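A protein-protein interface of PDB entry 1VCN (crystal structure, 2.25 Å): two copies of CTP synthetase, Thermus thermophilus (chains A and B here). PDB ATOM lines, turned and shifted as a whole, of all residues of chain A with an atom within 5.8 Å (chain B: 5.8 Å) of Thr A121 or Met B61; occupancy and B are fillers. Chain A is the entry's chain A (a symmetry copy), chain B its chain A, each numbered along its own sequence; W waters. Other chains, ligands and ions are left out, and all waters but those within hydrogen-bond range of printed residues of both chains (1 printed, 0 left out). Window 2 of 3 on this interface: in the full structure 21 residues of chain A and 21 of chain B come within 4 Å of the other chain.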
ATOM      1  N   SER A 119      29.206   2.102  25.456  1.00  0.00           N
ATOM      2  CA  SER A 119      28.017   2.830  25.006  1.00  0.00           C
ATOM      3  C   SER A 119      27.095   3.378  26.093  1.00  0.00           C
ATOM      4  O   SER A 119      25.911   3.598  25.840  1.00  0.00           O
ATOM      5  CB  SER A 119      27.183   1.948  24.069  1.00  0.00           C
ATOM      6  OG  SER A 119      27.923   1.561  22.924  1.00  0.00           O
ATOM      7  N   GLN A 120      27.613   3.595  27.296  1.00  0.00           N
ATOM      8  CA  GLN A 120      26.751   3.917  28.436  1.00  0.00           C
ATOM      9  C   GLN A 120      26.797   5.440  28.388  1.00  0.00           C
ATOM     10  O   GLN A 120      27.663   6.036  27.738  1.00  0.00           O
ATOM     11  CB  GLN A 120      27.283   3.467  29.799  1.00  0.00           C
ATOM     12  CG  GLN A 120      27.391   1.963  29.991  1.00  0.00           C
ATOM     13  CD  GLN A 120      28.113   1.599  31.281  1.00  0.00           C
ATOM     14  OE1 GLN A 120      28.829   0.592  31.346  1.00  0.00           O
ATOM     15  NE2 GLN A 120      27.925   2.415  32.319  1.00  0.00           N
ATOM     16  N   THR A 121      25.848   6.063  29.080  1.00  0.00           N
ATOM     17  CA  THR A 121      25.785   7.511  29.185  1.00  0.00           C
ATOM     18  C   THR A 121      26.476   7.825  30.501  1.00  0.00           C
ATOM     19  O   THR A 121      25.968   7.490  31.573  1.00  0.00           O
ATOM     20  CB  THR A 121      24.338   8.007  29.238  1.00  0.00           C
ATOM     21  OG1 THR A 121      23.684   7.661  28.010  1.00  0.00           O
ATOM     22  CG2 THR A 121      24.296   9.517  29.436  1.00  0.00           C
ATOM     23  N   VAL A 122      27.640   8.456  30.404  1.00  0.00           N
ATOM     24  CA  VAL A 122      28.451   8.793  31.565  1.00  0.00           C
ATOM     25  C   VAL A 122      27.951  10.008  32.339  1.00  0.00           C
ATOM     26  O   VAL A 122      27.750  11.082  31.779  1.00  0.00           O
ATOM     27  CB  VAL A 122      29.910   9.025  31.131  1.00  0.00           C
ATOM     28  CG1 VAL A 122      30.802   9.197  32.345  1.00  0.00           C
ATOM     29  CG2 VAL A 122      30.378   7.844  30.260  1.00  0.00           C
ATOM     30  N   GLN A 123      27.755   9.834  33.639  1.00  0.00           N
ATOM     31  CA  GLN A 123      27.278  10.926  34.478  1.00  0.00           C
ATOM     32  C   GLN A 123      28.216  11.133  35.652  1.00  0.00           C
ATOM     33  O   GLN A 123      29.072  10.290  35.936  1.00  0.00           O
ATOM     34  CB  GLN A 123      25.883  10.619  35.018  1.00  0.00           C
ATOM     35  CG  GLN A 123      24.834  10.266  33.971  1.00  0.00           C
ATOM     36  CD  GLN A 123      24.320  11.470  33.205  1.00  0.00           C
ATOM     37  OE1 GLN A 123      23.322  11.378  32.487  1.00  0.00           O
ATOM     38  NE2 GLN A 123      25.000  12.609  33.348  1.00  0.00           N
ATOM     39  N   HIS A 127      29.727   7.521  37.562  1.00  0.00           N
ATOM     40  CA  HIS A 127      31.028   7.499  36.887  1.00  0.00           C
ATOM     41  C   HIS A 127      32.151   8.356  37.471  1.00  0.00           C
ATOM     42  O   HIS A 127      33.255   7.860  37.667  1.00  0.00           O
ATOM     43  CB  HIS A 127      30.846   7.803  35.395  1.00  0.00           C
ATOM     44  CG  HIS A 127      29.758   6.999  34.763  1.00  0.00           C
ATOM     45  ND1 HIS A 127      28.424   7.304  34.926  1.00  0.00           N
ATOM     46  CD2 HIS A 127      29.796   5.856  34.039  1.00  0.00           C
ATOM     47  CE1 HIS A 127      27.687   6.386  34.328  1.00  0.00           C
ATOM     48  NE2 HIS A 127      28.496   5.496  33.783  1.00  0.00           N
ATOM     49  N   TYR B  53      25.610  15.325  30.447  1.00  0.00           N
ATOM     50  CA  TYR B  53      26.380  14.110  30.647  1.00  0.00           C
ATOM     51  C   TYR B  53      27.865  14.372  30.370  1.00  0.00           C
ATOM     52  O   TYR B  53      28.226  15.362  29.722  1.00  0.00           O
ATOM     53  CB  TYR B  53      25.835  12.936  29.802  1.00  0.00           C
ATOM     54  CG  TYR B  53      25.610  13.155  28.320  1.00  0.00           C
ATOM     55  CD1 TYR B  53      26.637  13.587  27.482  1.00  0.00           C
ATOM     56  CD2 TYR B  53      24.381  12.850  27.741  1.00  0.00           C
ATOM     57  CE1 TYR B  53      26.447  13.700  26.112  1.00  0.00           C
ATOM     58  CE2 TYR B  53      24.178  12.962  26.363  1.00  0.00           C
ATOM     59  CZ  TYR B  53      25.217  13.384  25.556  1.00  0.00           C
ATOM     60  OH  TYR B  53      25.038  13.458  24.193  1.00  0.00           O
ATOM     61  N   ASN B  55      29.886  12.597  28.529  1.00  0.00           N
ATOM     62  CA  ASN B  55      30.310  12.210  27.179  1.00  0.00           C
ATOM     63  C   ASN B  55      30.652  13.460  26.357  1.00  0.00           C
ATOM     64  O   ASN B  55      29.903  14.430  26.369  1.00  0.00           O
ATOM     65  CB  ASN B  55      29.189  11.431  26.480  1.00  0.00           C
ATOM     66  CG  ASN B  55      28.843  10.146  27.192  1.00  0.00           C
ATOM     67  OD1 ASN B  55      29.247   9.056  26.767  1.00  0.00           O
ATOM     68  ND2 ASN B  55      28.101  10.262  28.291  1.00  0.00           N
ATOM     69  N   ASP B  57      30.622  13.852  23.123  1.00  0.00           N
ATOM     70  CA  ASP B  57      29.535  13.978  22.157  1.00  0.00           C
ATOM     71  C   ASP B  57      28.725  12.693  22.207  1.00  0.00           C
ATOM     72  O   ASP B  57      28.942  11.866  23.098  1.00  0.00           O
ATOM     73  CB  ASP B  57      30.026  14.242  20.726  1.00  0.00           C
ATOM     74  CG  ASP B  57      30.936  13.166  20.199  1.00  0.00           C
ATOM     75  OD1 ASP B  57      30.701  11.975  20.475  1.00  0.00           O
ATOM     76  OD2 ASP B  57      31.889  13.527  19.479  1.00  0.00           O
ATOM     77  N   ALA B  58      27.811  12.512  21.257  1.00  0.00           N
ATOM     78  CA  ALA B  58      26.945  11.335  21.245  1.00  0.00           C
ATOM     79  C   ALA B  58      27.445  10.153  20.408  1.00  0.00           C
ATOM     80  O   ALA B  58      26.705   9.201  20.182  1.00  0.00           O
ATOM     81  CB  ALA B  58      25.542  11.740  20.779  1.00  0.00           C
ATOM     82  N   GLY B  59      28.695  10.210  19.969  1.00  0.00           N
ATOM     83  CA  GLY B  59      29.241   9.144  19.146  1.00  0.00           C
ATOM     84  C   GLY B  59      29.540   7.818  19.830  1.00  0.00           C
ATOM     85  O   GLY B  59      29.647   6.793  19.157  1.00  0.00           O
ATOM     86  N   THR B  60      29.684   7.825  21.151  1.00  0.00           N
ATOM     87  CA  THR B  60      29.978   6.593  21.879  1.00  0.00           C
ATOM     88  C   THR B  60      28.697   5.950  22.389  1.00  0.00           C
ATOM     89  O   THR B  60      28.734   4.932  23.072  1.00  0.00           O
ATOM     90  CB  THR B  60      30.911   6.855  23.093  1.00  0.00           C
ATOM     91  OG1 THR B  60      30.291   7.791  23.987  1.00  0.00           O
ATOM     92  CG2 THR B  60      32.256   7.405  22.633  1.00  0.00           C
ATOM     93  N   MET B  61      27.564   6.561  22.057  1.00  0.00           N
ATOM     94  CA  MET B  61      26.254   6.077  22.480  1.00  0.00           C
ATOM     95  C   MET B  61      25.826   4.832  21.706  1.00  0.00           C
ATOM     96  O   MET B  61      25.142   3.970  22.303  1.00  0.00           O
ATOM     97  CB  MET B  61      25.212   7.178  22.290  1.00  0.00           C
ATOM     98  CG  MET B  61      25.555   8.465  22.994  1.00  0.00           C
ATOM     99  SD  MET B  61      25.562   8.262  24.772  1.00  0.00           S
ATOM    100  CE  MET B  61      24.606   9.681  25.227  1.00  0.00           C
ATOM    101  N   GLY B  67      18.343   5.526  21.571  1.00  0.00           N
ATOM    102  CA  GLY B  67      17.910   6.741  20.832  1.00  0.00           C
ATOM    103  C   GLY B  67      18.868   7.078  19.712  1.00  0.00           C
ATOM    104  O   GLY B  67      20.072   6.877  19.837  1.00  0.00           O
ATOM    105  N   VAL B  69      21.312   8.921  17.012  1.00  0.00           N
ATOM    106  CA  VAL B  69      22.401   9.859  17.118  1.00  0.00           C
ATOM    107  C   VAL B  69      22.198  10.668  15.851  1.00  0.00           C
ATOM    108  O   VAL B  69      22.264  10.122  14.751  1.00  0.00           O
ATOM    109  CB  VAL B  69      23.759   9.150  17.067  1.00  0.00           C
ATOM    110  CG1 VAL B  69      24.882  10.172  16.957  1.00  0.00           C
ATOM    111  CG2 VAL B  69      23.934   8.292  18.311  1.00  0.00           C
HETATM  112  O   HOH W   1      30.262   5.323  26.353  1.00  0.00           O
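O of Thr B60 lies close to OG of Ser A119, at 3.5 Å. SD of Met B61 sits close to OG1 of Thr A121, 3.8 Å away. The backbone NH of Val A122 lies close to the side-chain amide nitrogen of Asn B55 (2.8 Å).
The backbone NH of Gln A123 lies within hydrogen-bond range of a ring nitrogen (ND1) of His A127 (2.9 Å). The side-chain amide oxygen of Asn B55 lies within hydrogen-bond range of the side-chain hydroxyl of Thr B60 (3.2 Å). A ring nitrogen (NE2) of His A127 is in hydrogen-bond range of the side-chain amide nitrogen (NE2) of Gln A120 (3.5 Å).
Among the printed residues, pairs that only touch across the chains: Val A122 with Tyr B53 (3.3 Å), Ser A119 with Met B61 (3.4 Å), Gln A123 with Tyr B53 (3.4 Å), Gln A120 with Asn B55 (3.5 Å), Thr A121 with Asn B55 (3.7 Å) and Thr A121 with Tyr B53 (3.7 Å).
Printed residues of chain B within 4 Å of Ser A119: Thr B60 and Met B61. Of the printed residues of chain B, Gln A120 touches Asn B55. Thr A121 touches just these residues of chain B: Tyr B53, Asn B55 and Met B61. Ala B58 touches none of the printed residues of chain A. Of the printed residues of chain A, Thr B60 touches Ser A119 (2.9 Å). Of chain A, only Ser A119 (3.4 Å) and Thr A121 (3.6 Å) come within 4 Å of Met B61. Val B69 touches none of the printed residues of chain A. The nearest printed residue of chain B that does not touch Thr A121 is Thr B60 (6.8 Å).
Of the 9 printed residues of chain B, 4 touch a printed residue of chain A. Hydrophobic or aromatic side chains of chain B that line the printed part of chain A: Tyr B53 and Met B61. Of the 6 printed residues of chain A, 5 touch a printed residue of chain B. Printed residues of chain A that touch a printed residue of chain B: Ser A119, Gln A120, Thr A121, Val A122 and Gln A123. Hydrophobic or aromatic side chains of chain A within 4 Å of the printed part of chain B: Val A122.
No position is printed for both chains. Of the 9 pairs that touch across the chains among the printed residues, none has its exchanged pair printed and touching as well.
Water W1 lies within hydrogen-bond range of O of Gln A120 (3.0 Å) and OG1 of Thr B60 (3.4 Å).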
